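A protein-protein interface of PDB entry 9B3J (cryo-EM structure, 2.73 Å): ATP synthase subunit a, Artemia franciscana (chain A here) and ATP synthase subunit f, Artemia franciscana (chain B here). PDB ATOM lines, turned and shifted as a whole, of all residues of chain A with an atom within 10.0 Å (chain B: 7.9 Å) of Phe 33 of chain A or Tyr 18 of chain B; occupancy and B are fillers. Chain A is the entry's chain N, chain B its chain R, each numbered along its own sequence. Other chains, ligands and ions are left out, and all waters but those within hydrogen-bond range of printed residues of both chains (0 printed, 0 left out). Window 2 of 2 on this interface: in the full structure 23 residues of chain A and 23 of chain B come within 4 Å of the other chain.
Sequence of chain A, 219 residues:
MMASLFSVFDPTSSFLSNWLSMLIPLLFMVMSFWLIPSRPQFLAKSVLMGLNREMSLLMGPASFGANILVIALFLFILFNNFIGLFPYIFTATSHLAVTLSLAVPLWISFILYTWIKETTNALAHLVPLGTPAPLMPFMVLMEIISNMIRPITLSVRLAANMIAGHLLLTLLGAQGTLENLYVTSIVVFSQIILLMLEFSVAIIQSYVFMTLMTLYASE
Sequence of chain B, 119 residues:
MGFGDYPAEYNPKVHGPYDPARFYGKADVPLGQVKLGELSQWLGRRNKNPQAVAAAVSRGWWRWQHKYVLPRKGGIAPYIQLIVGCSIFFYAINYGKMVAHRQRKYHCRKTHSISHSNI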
ATOM      1  N   MET A  29      32.881  19.369   3.067  1.00  0.00           N
ATOM      2  CA  MET A  29      32.758  19.877   4.425  1.00  0.00           C
ATOM      3  C   MET A  29      32.562  18.704   5.369  1.00  0.00           C
ATOM      4  O   MET A  29      31.749  17.814   5.103  1.00  0.00           O
ATOM      5  CB  MET A  29      31.593  20.857   4.545  1.00  0.00           C
ATOM      6  CG  MET A  29      31.429  21.459   5.929  1.00  0.00           C
ATOM      7  SD  MET A  29      32.839  22.446   6.458  1.00  0.00           S
ATOM      8  CE  MET A  29      32.941  23.610   5.108  1.00  0.00           C
ATOM      9  N   VAL A  30      33.313  18.709   6.470  1.00  0.00           N
ATOM     10  CA  VAL A  30      33.358  17.561   7.363  1.00  0.00           C
ATOM     11  C   VAL A  30      32.060  17.462   8.147  1.00  0.00           C
ATOM     12  O   VAL A  30      31.560  18.455   8.688  1.00  0.00           O
ATOM     13  CB  VAL A  30      34.569  17.665   8.293  1.00  0.00           C
ATOM     14  CG1 VAL A  30      35.797  17.227   7.553  1.00  0.00           C
ATOM     15  CG2 VAL A  30      34.743  19.084   8.751  1.00  0.00           C
ATOM     16  N   MET A  31      31.499  16.262   8.192  1.00  0.00           N
ATOM     17  CA  MET A  31      30.306  15.987   8.971  1.00  0.00           C
ATOM     18  C   MET A  31      30.705  15.301  10.266  1.00  0.00           C
ATOM     19  O   MET A  31      31.543  14.397  10.267  1.00  0.00           O
ATOM     20  CB  MET A  31      29.330  15.113   8.188  1.00  0.00           C
ATOM     21  CG  MET A  31      28.413  15.887   7.263  1.00  0.00           C
ATOM     22  SD  MET A  31      27.282  14.780   6.406  1.00  0.00           S
ATOM     23  CE  MET A  31      26.195  15.947   5.607  1.00  0.00           C
ATOM     24  N   SER A  32      30.096  15.736  11.365  1.00  0.00           N
ATOM     25  CA  SER A  32      30.471  15.311  12.706  1.00  0.00           C
ATOM     26  C   SER A  32      29.401  14.391  13.271  1.00  0.00           C
ATOM     27  O   SER A  32      28.240  14.783  13.386  1.00  0.00           O
ATOM     28  CB  SER A  32      30.676  16.520  13.611  1.00  0.00           C
ATOM     29  OG  SER A  32      29.587  17.415  13.507  1.00  0.00           O
ATOM     30  N   PHE A  33      29.795  13.174  13.623  1.00  0.00           N
ATOM     31  CA  PHE A  33      28.904  12.200  14.233  1.00  0.00           C
ATOM     32  C   PHE A  33      29.358  11.787  15.621  1.00  0.00           C
ATOM     33  O   PHE A  33      28.575  11.871  16.571  1.00  0.00           O
ATOM     34  CB  PHE A  33      28.791  10.969  13.331  1.00  0.00           C
ATOM     35  CG  PHE A  33      27.890   9.904  13.858  1.00  0.00           C
ATOM     36  CD1 PHE A  33      26.543   9.965  13.645  1.00  0.00           C
ATOM     37  CD2 PHE A  33      28.397   8.816  14.517  1.00  0.00           C
ATOM     38  CE1 PHE A  33      25.717   8.978  14.109  1.00  0.00           C
ATOM     39  CE2 PHE A  33      27.571   7.831  14.984  1.00  0.00           C
ATOM     40  CZ  PHE A  33      26.233   7.913  14.777  1.00  0.00           C
ATOM     41  N   TRP A  34      30.599  11.339  15.772  1.00  0.00           N
ATOM     42  CA  TRP A  34      31.038  10.850  17.067  1.00  0.00           C
ATOM     43  C   TRP A  34      31.514  11.999  17.943  1.00  0.00           C
ATOM     44  O   TRP A  34      31.818  13.094  17.466  1.00  0.00           O
ATOM     45  CB  TRP A  34      32.157   9.830  16.915  1.00  0.00           C
ATOM     46  CG  TRP A  34      31.781   8.607  16.171  1.00  0.00           C
ATOM     47  CD1 TRP A  34      32.102   8.310  14.890  1.00  0.00           C
ATOM     48  CD2 TRP A  34      31.019   7.503  16.661  1.00  0.00           C
ATOM     49  NE1 TRP A  34      31.589   7.089  14.546  1.00  0.00           N
ATOM     50  CE2 TRP A  34      30.918   6.574  15.621  1.00  0.00           C
ATOM     51  CE3 TRP A  34      30.415   7.211  17.879  1.00  0.00           C
ATOM     52  CZ2 TRP A  34      30.241   5.378  15.758  1.00  0.00           C
ATOM     53  CZ3 TRP A  34      29.746   6.021  18.011  1.00  0.00           C
ATOM     54  CH2 TRP A  34      29.662   5.121  16.959  1.00  0.00           C
ATOM     55  N   LEU A  35      31.577  11.733  19.248  1.00  0.00           N
ATOM     56  CA  LEU A  35      31.947  12.776  20.197  1.00  0.00           C
ATOM     57  C   LEU A  35      33.417  13.136  20.071  1.00  0.00           C
ATOM     58  O   LEU A  35      33.776  14.317  20.028  1.00  0.00           O
ATOM     59  CB  LEU A  35      31.623  12.331  21.618  1.00  0.00           C
ATOM     60  CG  LEU A  35      32.052  13.289  22.720  1.00  0.00           C
ATOM     61  CD1 LEU A  35      31.339  14.613  22.587  1.00  0.00           C
ATOM     62  CD2 LEU A  35      31.758  12.661  24.055  1.00  0.00           C
ATOM     63  N   ILE A  36      34.284  12.132  20.020  1.00  0.00           N
ATOM     64  CA  ILE A  36      35.703  12.350  19.766  1.00  0.00           C
ATOM     65  C   ILE A  36      35.882  12.410  18.258  1.00  0.00           C
ATOM     66  O   ILE A  36      35.515  11.461  17.557  1.00  0.00           O
ATOM     67  CB  ILE A  36      36.564  11.250  20.398  1.00  0.00           C
ATOM     68  CG1 ILE A  36      35.803   9.926  20.396  1.00  0.00           C
ATOM     69  CG2 ILE A  36      36.956  11.634  21.808  1.00  0.00           C
ATOM     70  CD1 ILE A  36      36.630   8.763  20.856  1.00  0.00           C
ATOM     71  N   PRO A  37      36.422  13.493  17.719  1.00  0.00           N
ATOM     72  CA  PRO A  37      36.387  13.694  16.269  1.00  0.00           C
ATOM     73  C   PRO A  37      37.342  12.762  15.542  1.00  0.00           C
ATOM     74  O   PRO A  37      38.203  12.115  16.134  1.00  0.00           O
ATOM     75  CB  PRO A  37      36.798  15.159  16.104  1.00  0.00           C
ATOM     76  CG  PRO A  37      37.499  15.514  17.344  1.00  0.00           C
ATOM     77  CD  PRO A  37      36.993  14.641  18.435  1.00  0.00           C
ATOM     78  N   SER A  38      37.153  12.674  14.232  1.00  0.00           N
ATOM     79  CA  SER A  38      38.082  11.936  13.395  1.00  0.00           C
ATOM     80  C   SER A  38      39.266  12.824  13.044  1.00  0.00           C
ATOM     81  O   SER A  38      39.368  13.969  13.488  1.00  0.00           O
ATOM     82  CB  SER A  38      37.384  11.434  12.140  1.00  0.00           C
ATOM     83  OG  SER A  38      36.841  12.517  11.413  1.00  0.00           O
ATOM     84  N   GLN A  41      37.973  15.917  10.624  1.00  0.00           N
ATOM     85  CA  GLN A  41      37.166  16.861  11.384  1.00  0.00           C
ATOM     86  C   GLN A  41      38.023  17.650  12.357  1.00  0.00           C
ATOM     87  O   GLN A  41      37.862  18.867  12.489  1.00  0.00           O
ATOM     88  CB  GLN A  41      36.065  16.124  12.131  1.00  0.00           C
ATOM     89  CG  GLN A  41      35.221  17.025  12.990  1.00  0.00           C
ATOM     90  CD  GLN A  41      34.285  16.255  13.879  1.00  0.00           C
ATOM     91  OE1 GLN A  41      34.035  15.068  13.667  1.00  0.00           O
ATOM     92  NE2 GLN A  41      33.772  16.922  14.900  1.00  0.00           N
ATOM     93  N   PHE A  42      38.950  16.976  13.037  1.00  0.00           N
ATOM     94  CA  PHE A  42      39.834  17.676  13.958  1.00  0.00           C
ATOM     95  C   PHE A  42      40.756  18.629  13.218  1.00  0.00           C
ATOM     96  O   PHE A  42      41.018  19.735  13.698  1.00  0.00           O
ATOM     97  CB  PHE A  42      40.651  16.688  14.781  1.00  0.00           C
ATOM     98  CG  PHE A  42      41.661  17.347  15.668  1.00  0.00           C
ATOM     99  CD1 PHE A  42      41.261  18.000  16.814  1.00  0.00           C
ATOM    100  CD2 PHE A  42      43.006  17.334  15.347  1.00  0.00           C
ATOM    101  CE1 PHE A  42      42.181  18.620  17.628  1.00  0.00           C
ATOM    102  CE2 PHE A  42      43.929  17.954  16.156  1.00  0.00           C
ATOM    103  CZ  PHE A  42      43.516  18.596  17.299  1.00  0.00           C
ATOM    104  N   ASP B   5      14.537  17.549  11.328  1.00  0.00           N
ATOM    105  CA  ASP B   5      13.777  16.724  12.257  1.00  0.00           C
ATOM    106  C   ASP B   5      14.129  15.300  11.888  1.00  0.00           C
ATOM    107  O   ASP B   5      14.490  15.033  10.740  1.00  0.00           O
ATOM    108  CB  ASP B   5      12.259  16.954  12.125  1.00  0.00           C
ATOM    109  CG  ASP B   5      11.476  16.676  13.416  1.00  0.00           C
ATOM    110  OD1 ASP B   5      12.052  16.223  14.428  1.00  0.00           O
ATOM    111  OD2 ASP B   5      10.254  16.936  13.406  1.00  0.00           O
ATOM    112  N   TYR B   6      14.040  14.394  12.847  1.00  0.00           N
ATOM    113  CA  TYR B   6      14.270  13.004  12.512  1.00  0.00           C
ATOM    114  C   TYR B   6      13.112  12.500  11.659  1.00  0.00           C
ATOM    115  O   TYR B   6      12.005  13.035  11.735  1.00  0.00           O
ATOM    116  CB  TYR B   6      14.404  12.152  13.769  1.00  0.00           C
ATOM    117  CG  TYR B   6      15.372  12.694  14.794  1.00  0.00           C
ATOM    118  CD1 TYR B   6      16.571  13.278  14.417  1.00  0.00           C
ATOM    119  CD2 TYR B   6      15.077  12.629  16.143  1.00  0.00           C
ATOM    120  CE1 TYR B   6      17.443  13.778  15.356  1.00  0.00           C
ATOM    121  CE2 TYR B   6      15.943  13.119  17.086  1.00  0.00           C
ATOM    122  CZ  TYR B   6      17.121  13.694  16.687  1.00  0.00           C
ATOM    123  OH  TYR B   6      17.986  14.188  17.627  1.00  0.00           O
ATOM    124  N   PRO B   7      13.347  11.511  10.803  1.00  0.00           N
ATOM    125  CA  PRO B   7      12.240  10.926  10.044  1.00  0.00           C
ATOM    126  C   PRO B   7      11.243  10.247  10.966  1.00  0.00           C
ATOM    127  O   PRO B   7      11.583   9.795  12.059  1.00  0.00           O
ATOM    128  CB  PRO B   7      12.931   9.916   9.122  1.00  0.00           C
ATOM    129  CG  PRO B   7      14.280   9.720   9.706  1.00  0.00           C
ATOM    130  CD  PRO B   7      14.643  11.021  10.319  1.00  0.00           C
ATOM    131  N   GLU B   9       9.730   7.476  11.000  1.00  0.00           N
ATOM    132  CA  GLU B   9       9.915   6.086  11.380  1.00  0.00           C
ATOM    133  C   GLU B   9      10.920   5.910  12.508  1.00  0.00           C
ATOM    134  O   GLU B   9      10.975   4.826  13.097  1.00  0.00           O
ATOM    135  CB  GLU B   9      10.355   5.270  10.164  1.00  0.00           C
ATOM    136  CG  GLU B   9       9.318   5.184   9.048  1.00  0.00           C
ATOM    137  CD  GLU B   9       9.409   6.328   8.048  1.00  0.00           C
ATOM    138  OE1 GLU B   9       9.538   7.495   8.471  1.00  0.00           O
ATOM    139  OE2 GLU B   9       9.352   6.054   6.831  1.00  0.00           O
ATOM    140  N   TYR B  10      11.698   6.940  12.831  1.00  0.00           N
ATOM    141  CA  TYR B  10      12.702   6.823  13.880  1.00  0.00           C
ATOM    142  C   TYR B  10      12.049   6.801  15.253  1.00  0.00           C
ATOM    143  O   TYR B  10      11.266   7.691  15.596  1.00  0.00           O
ATOM    144  CB  TYR B  10      13.692   7.979  13.796  1.00  0.00           C
ATOM    145  CG  TYR B  10      14.598   8.092  14.997  1.00  0.00           C
ATOM    146  CD1 TYR B  10      15.501   7.088  15.304  1.00  0.00           C
ATOM    147  CD2 TYR B  10      14.560   9.206  15.815  1.00  0.00           C
ATOM    148  CE1 TYR B  10      16.332   7.188  16.397  1.00  0.00           C
ATOM    149  CE2 TYR B  10      15.388   9.314  16.908  1.00  0.00           C
ATOM    150  CZ  TYR B  10      16.272   8.305  17.193  1.00  0.00           C
ATOM    151  OH  TYR B  10      17.098   8.413  18.284  1.00  0.00           O
ATOM    152  N   ASN B  11      12.382   5.786  16.043  1.00  0.00           N
ATOM    153  CA  ASN B  11      11.873   5.648  17.408  1.00  0.00           C
ATOM    154  C   ASN B  11      13.050   5.561  18.367  1.00  0.00           C
ATOM    155  O   ASN B  11      13.701   4.505  18.457  1.00  0.00           O
ATOM    156  CB  ASN B  11      10.986   4.413  17.532  1.00  0.00           C
ATOM    157  CG  ASN B  11      10.053   4.484  18.719  1.00  0.00           C
ATOM    158  OD1 ASN B  11      10.350   5.124  19.728  1.00  0.00           O
ATOM    159  ND2 ASN B  11       8.909   3.823  18.604  1.00  0.00           N
ATOM    160  N   PRO B  12      13.362   6.635  19.100  1.00  0.00           N
ATOM    161  CA  PRO B  12      14.525   6.600  20.003  1.00  0.00           C
ATOM    162  C   PRO B  12      14.386   5.621  21.153  1.00  0.00           C
ATOM    163  O   PRO B  12      15.402   5.260  21.758  1.00  0.00           O
ATOM    164  CB  PRO B  12      14.617   8.044  20.509  1.00  0.00           C
ATOM    165  CG  PRO B  12      13.245   8.588  20.344  1.00  0.00           C
ATOM    166  CD  PRO B  12      12.691   7.942  19.115  1.00  0.00           C
ATOM    167  N   HIS B  15      14.934   2.077  18.511  1.00  0.00           N
ATOM    168  CA  HIS B  15      16.085   1.951  17.631  1.00  0.00           C
ATOM    169  C   HIS B  15      17.386   2.437  18.253  1.00  0.00           C
ATOM    170  O   HIS B  15      18.415   2.433  17.572  1.00  0.00           O
ATOM    171  CB  HIS B  15      15.831   2.715  16.333  1.00  0.00           C
ATOM    172  CG  HIS B  15      14.632   2.237  15.578  1.00  0.00           C
ATOM    173  ND1 HIS B  15      13.387   2.808  15.723  1.00  0.00           N
ATOM    174  CD2 HIS B  15      14.487   1.241  14.674  1.00  0.00           C
ATOM    175  CE1 HIS B  15      12.526   2.186  14.938  1.00  0.00           C
ATOM    176  NE2 HIS B  15      13.168   1.230  14.290  1.00  0.00           N
ATOM    177  N   GLY B  16      17.377   2.857  19.510  1.00  0.00           N
ATOM    178  CA  GLY B  16      18.576   3.364  20.131  1.00  0.00           C
ATOM    179  C   GLY B  16      18.957   4.729  19.599  1.00  0.00           C
ATOM    180  O   GLY B  16      18.104   5.511  19.169  1.00  0.00           O
ATOM    181  N   PRO B  17      20.249   5.043  19.623  1.00  0.00           N
ATOM    182  CA  PRO B  17      20.702   6.349  19.138  1.00  0.00           C
ATOM    183  C   PRO B  17      20.532   6.471  17.634  1.00  0.00           C
ATOM    184  O   PRO B  17      20.426   5.481  16.907  1.00  0.00           O
ATOM    185  CB  PRO B  17      22.180   6.381  19.530  1.00  0.00           C
ATOM    186  CG  PRO B  17      22.571   4.964  19.585  1.00  0.00           C
ATOM    187  CD  PRO B  17      21.369   4.216  20.092  1.00  0.00           C
ATOM    188  N   TYR B  18      20.497   7.718  17.174  1.00  0.00           N
ATOM    189  CA  TYR B  18      20.158   8.002  15.788  1.00  0.00           C
ATOM    190  C   TYR B  18      21.360   7.739  14.897  1.00  0.00           C
ATOM    191  O   TYR B  18      22.396   8.399  15.030  1.00  0.00           O
ATOM    192  CB  TYR B  18      19.682   9.442  15.635  1.00  0.00           C
ATOM    193  CG  TYR B  18      19.216   9.772  14.243  1.00  0.00           C
ATOM    194  CD1 TYR B  18      18.268   8.987  13.604  1.00  0.00           C
ATOM    195  CD2 TYR B  18      19.712  10.875  13.573  1.00  0.00           C
ATOM    196  CE1 TYR B  18      17.839   9.286  12.331  1.00  0.00           C
ATOM    197  CE2 TYR B  18      19.285  11.183  12.301  1.00  0.00           C
ATOM    198  CZ  TYR B  18      18.348  10.387  11.686  1.00  0.00           C
ATOM    199  OH  TYR B  18      17.923  10.693  10.417  1.00  0.00           O
ATOM    200  N   ASP B  19      21.213   6.776  13.988  1.00  0.00           N
ATOM    201  CA  ASP B  19      22.233   6.430  13.006  1.00  0.00           C
ATOM    202  C   ASP B  19      21.719   6.854  11.643  1.00  0.00           C
ATOM    203  O   ASP B  19      20.906   6.139  11.041  1.00  0.00           O
ATOM    204  CB  ASP B  19      22.512   4.926  13.028  1.00  0.00           C
ATOM    205  CG  ASP B  19      23.725   4.546  12.211  1.00  0.00           C
ATOM    206  OD1 ASP B  19      24.463   5.455  11.773  1.00  0.00           O
ATOM    207  OD2 ASP B  19      23.941   3.331  12.008  1.00  0.00           O
ATOM    208  N   PRO B  20      22.157   8.000  11.115  1.00  0.00           N
ATOM    209  CA  PRO B  20      21.516   8.546   9.912  1.00  0.00           C
ATOM    210  C   PRO B  20      21.744   7.720   8.665  1.00  0.00           C
ATOM    211  O   PRO B  20      20.972   7.851   7.710  1.00  0.00           O
ATOM    212  CB  PRO B  20      22.139   9.942   9.786  1.00  0.00           C
ATOM    213  CG  PRO B  20      23.412   9.854  10.515  1.00  0.00           C
ATOM    214  CD  PRO B  20      23.204   8.890  11.633  1.00  0.00           C
ATOM    215  N   ALA B  21      22.755   6.861   8.643  1.00  0.00           N
ATOM    216  CA  ALA B  21      22.949   5.974   7.511  1.00  0.00           C
ATOM    217  C   ALA B  21      21.980   4.804   7.509  1.00  0.00           C
ATOM    218  O   ALA B  21      21.892   4.105   6.497  1.00  0.00           O
ATOM    219  CB  ALA B  21      24.380   5.445   7.498  1.00  0.00           C
ATOM    220  N   ARG B  22      21.259   4.571   8.598  1.00  0.00           N
ATOM    221  CA  ARG B  22      20.360   3.432   8.682  1.00  0.00           C
ATOM    222  C   ARG B  22      18.961   3.843   8.253  1.00  0.00           C
ATOM    223  O   ARG B  22      18.499   4.944   8.561  1.00  0.00           O
ATOM    224  CB  ARG B  22      20.340   2.864  10.103  1.00  0.00           C
ATOM    225  CG  ARG B  22      19.542   1.572  10.265  1.00  0.00           C
ATOM    226  CD  ARG B  22      19.410   1.169  11.732  1.00  0.00           C
ATOM    227  NE  ARG B  22      18.391   0.144  11.946  1.00  0.00           N
ATOM    228  CZ  ARG B  22      18.016  -0.311  13.135  1.00  0.00           C
ATOM    229  NH1 ARG B  22      18.560   0.139  14.253  1.00  0.00           N
ATOM    230  NH2 ARG B  22      17.066  -1.239  13.206  1.00  0.00           N
ATOM    231  N   TYR B  24      15.192   3.372   8.798  1.00  0.00           N
ATOM    232  CA  TYR B  24      14.389   2.940   9.934  1.00  0.00           C
ATOM    233  C   TYR B  24      12.992   2.477   9.550  1.00  0.00           C
ATOM    234  O   TYR B  24      12.210   2.132  10.439  1.00  0.00           O
ATOM    235  CB  TYR B  24      14.284   4.067  10.962  1.00  0.00           C
ATOM    236  CG  TYR B  24      15.585   4.385  11.654  1.00  0.00           C
ATOM    237  CD1 TYR B  24      16.106   3.531  12.614  1.00  0.00           C
ATOM    238  CD2 TYR B  24      16.285   5.543  11.356  1.00  0.00           C
ATOM    239  CE1 TYR B  24      17.291   3.816  13.249  1.00  0.00           C
ATOM    240  CE2 TYR B  24      17.469   5.836  11.989  1.00  0.00           C
ATOM    241  CZ  TYR B  24      17.965   4.968  12.935  1.00  0.00           C
ATOM    242  OH  TYR B  24      19.149   5.254  13.569  1.00  0.00           O
ATOM    243  N   SER B  58      20.891  10.714   0.965  1.00  0.00           N
ATOM    244  CA  SER B  58      21.511  11.066   2.237  1.00  0.00           C
ATOM    245  C   SER B  58      21.908   9.830   3.033  1.00  0.00           C
ATOM    246  O   SER B  58      22.940   9.832   3.712  1.00  0.00           O
ATOM    247  CB  SER B  58      20.573  11.936   3.057  1.00  0.00           C
ATOM    248  OG  SER B  58      21.200  12.309   4.266  1.00  0.00           O
ATOM    249  N   ARG B  59      21.108   8.770   2.967  1.00  0.00           N
ATOM    250  CA  ARG B  59      21.490   7.532   3.633  1.00  0.00           C
ATOM    251  C   ARG B  59      22.733   6.923   3.000  1.00  0.00           C
ATOM    252  O   ARG B  59      23.613   6.421   3.710  1.00  0.00           O
ATOM    253  CB  ARG B  59      20.337   6.540   3.608  1.00  0.00           C
ATOM    254  CG  ARG B  59      19.254   6.857   4.597  1.00  0.00           C
ATOM    255  CD  ARG B  59      18.198   5.783   4.597  1.00  0.00           C
ATOM    256  NE  ARG B  59      17.363   5.852   3.407  1.00  0.00           N
ATOM    257  CZ  ARG B  59      16.239   6.548   3.328  1.00  0.00           C
ATOM    258  NH1 ARG B  59      15.787   7.245   4.354  1.00  0.00           N
ATOM    259  NH2 ARG B  59      15.550   6.542   2.192  1.00  0.00           N
ATOM    260  N   TRP B  62      25.753   8.952   4.053  1.00  0.00           N
ATOM    261  CA  TRP B  62      26.170   8.657   5.416  1.00  0.00           C
ATOM    262  C   TRP B  62      26.783   7.268   5.550  1.00  0.00           C
ATOM    263  O   TRP B  62      27.631   7.067   6.420  1.00  0.00           O
ATOM    264  CB  TRP B  62      24.997   8.843   6.374  1.00  0.00           C
ATOM    265  CG  TRP B  62      24.944  10.241   6.865  1.00  0.00           C
ATOM    266  CD1 TRP B  62      24.211  11.260   6.352  1.00  0.00           C
ATOM    267  CD2 TRP B  62      25.705  10.794   7.942  1.00  0.00           C
ATOM    268  NE1 TRP B  62      24.453  12.411   7.050  1.00  0.00           N
ATOM    269  CE2 TRP B  62      25.370  12.149   8.032  1.00  0.00           C
ATOM    270  CE3 TRP B  62      26.630  10.270   8.844  1.00  0.00           C
ATOM    271  CZ2 TRP B  62      25.919  12.981   8.991  1.00  0.00           C
ATOM    272  CZ3 TRP B  62      27.176  11.100   9.784  1.00  0.00           C
ATOM    273  CH2 TRP B  62      26.823  12.439   9.849  1.00  0.00           C
ATOM    274  N   GLN B  65      30.244   8.019   4.521  1.00  0.00           N
ATOM    275  CA  GLN B  65      30.909   8.713   5.615  1.00  0.00           C
ATOM    276  C   GLN B  65      31.293   7.740   6.716  1.00  0.00           C
ATOM    277  O   GLN B  65      32.400   7.811   7.262  1.00  0.00           O
ATOM    278  CB  GLN B  65      30.009   9.817   6.163  1.00  0.00           C
ATOM    279  CG  GLN B  65      29.888  11.033   5.276  1.00  0.00           C
ATOM    280  CD  GLN B  65      31.003  12.018   5.478  1.00  0.00           C
ATOM    281  OE1 GLN B  65      31.790  11.890   6.402  1.00  0.00           O
ATOM    282  NE2 GLN B  65      31.074  13.018   4.617  1.00  0.00           N
ATOM    283  N   HIS B  66      30.404   6.799   7.030  1.00  0.00           N
ATOM    284  CA  HIS B  66      30.676   5.813   8.061  1.00  0.00           C
ATOM    285  C   HIS B  66      31.758   4.830   7.659  1.00  0.00           C
ATOM    286  O   HIS B  66      32.382   4.228   8.536  1.00  0.00           O
ATOM    287  CB  HIS B  66      29.405   5.048   8.401  1.00  0.00           C
ATOM    288  CG  HIS B  66      28.736   5.528   9.647  1.00  0.00           C
ATOM    289  ND1 HIS B  66      29.378   5.557  10.864  1.00  0.00           N
ATOM    290  CD2 HIS B  66      27.486   5.993   9.866  1.00  0.00           C
ATOM    291  CE1 HIS B  66      28.548   6.019  11.781  1.00  0.00           C
ATOM    292  NE2 HIS B  66      27.394   6.291  11.200  1.00  0.00           N
ATOM    293  N   LEU B  70      34.204   8.743   9.045  1.00  0.00           N
ATOM    294  CA  LEU B  70      33.883   8.712  10.470  1.00  0.00           C
ATOM    295  C   LEU B  70      34.746   7.793  11.342  1.00  0.00           C
ATOM    296  O   LEU B  70      34.814   8.062  12.553  1.00  0.00           O
ATOM    297  CB  LEU B  70      32.402   8.351  10.651  1.00  0.00           C
ATOM    298  CG  LEU B  70      31.408   9.389  10.141  1.00  0.00           C
ATOM    299  CD1 LEU B  70      29.996   8.914  10.379  1.00  0.00           C
ATOM    300  CD2 LEU B  70      31.646  10.718  10.809  1.00  0.00           C
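SD of Met 31 of chain A sits close to NE1 of Trp 62 of chain B, 3.7 Å away.
A ring nitrogen (NE2) of His 66 of chain B is in hydrogen-bond range of the side-chain carboxylate (OD1) of Asp 19 of chain B (3.1 Å).
The backbone NH (N) of Leu 70 of chain B sits at hydrogen-bond distance from the backbone carbonyl oxygen (O) of Gln 65 of chain B (2.7 Å).
Among the printed residues, merely in contact across the chains: Phe 33 of chain A with Tyr 18 of chain B (3.5 Å), Phe 33 of chain A with Pro 20 of chain B (3.5 Å), Trp 34 of chain A with Leu 70 of chain B (3.6 Å), Met 31 of chain A with Leu 70 of chain B (3.7 Å), Phe 33 of chain A with Leu 70 of chain B (3.8 Å), Phe 33 of chain A with His 66 of chain B (3.8 Å) and Phe 33 of chain A with Trp 62 of chain B (3.9 Å).
Phe 33 of chain A touches just these residues of chain B: Tyr 18 (3.5 Å), Pro 20 (3.5 Å), Trp 62 (3.9 Å), His 66 (3.8 Å) and Leu 70 (3.8 Å).
Tyr 18 of chain B touches just one residue of chain A: Phe 33 (3.5 Å).
No residue of chain A comes within 4 Å of Pro 17 of chain B.
No residue of chain A comes within 4 Å of Asp 19 of chain B.
Printed residues of chain A within 4 Å of Pro 20 of chain B: Phe 33.
Of the printed residues of chain B, Met 31 of chain A touches Trp 62 (3.4 Å) and Leu 70 (3.7 Å).
Of the printed residues of chain B, Trp 34 of chain A touches Leu 70.
Tyr 6 of chain B touches none of the printed residues of chain A.
Asp 5 of chain B touches none of the printed residues of chain A.
Printed residues of chain A that touch a printed residue of chain B: Met 31, Phe 33 and Trp 34.
Among the printed residues, 8 pairs touch across the chains.
Among the printed residues, no Asp or Glu carboxylate lies within 4 Å of a Lys or Arg side-chain nitrogen of the other chain.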
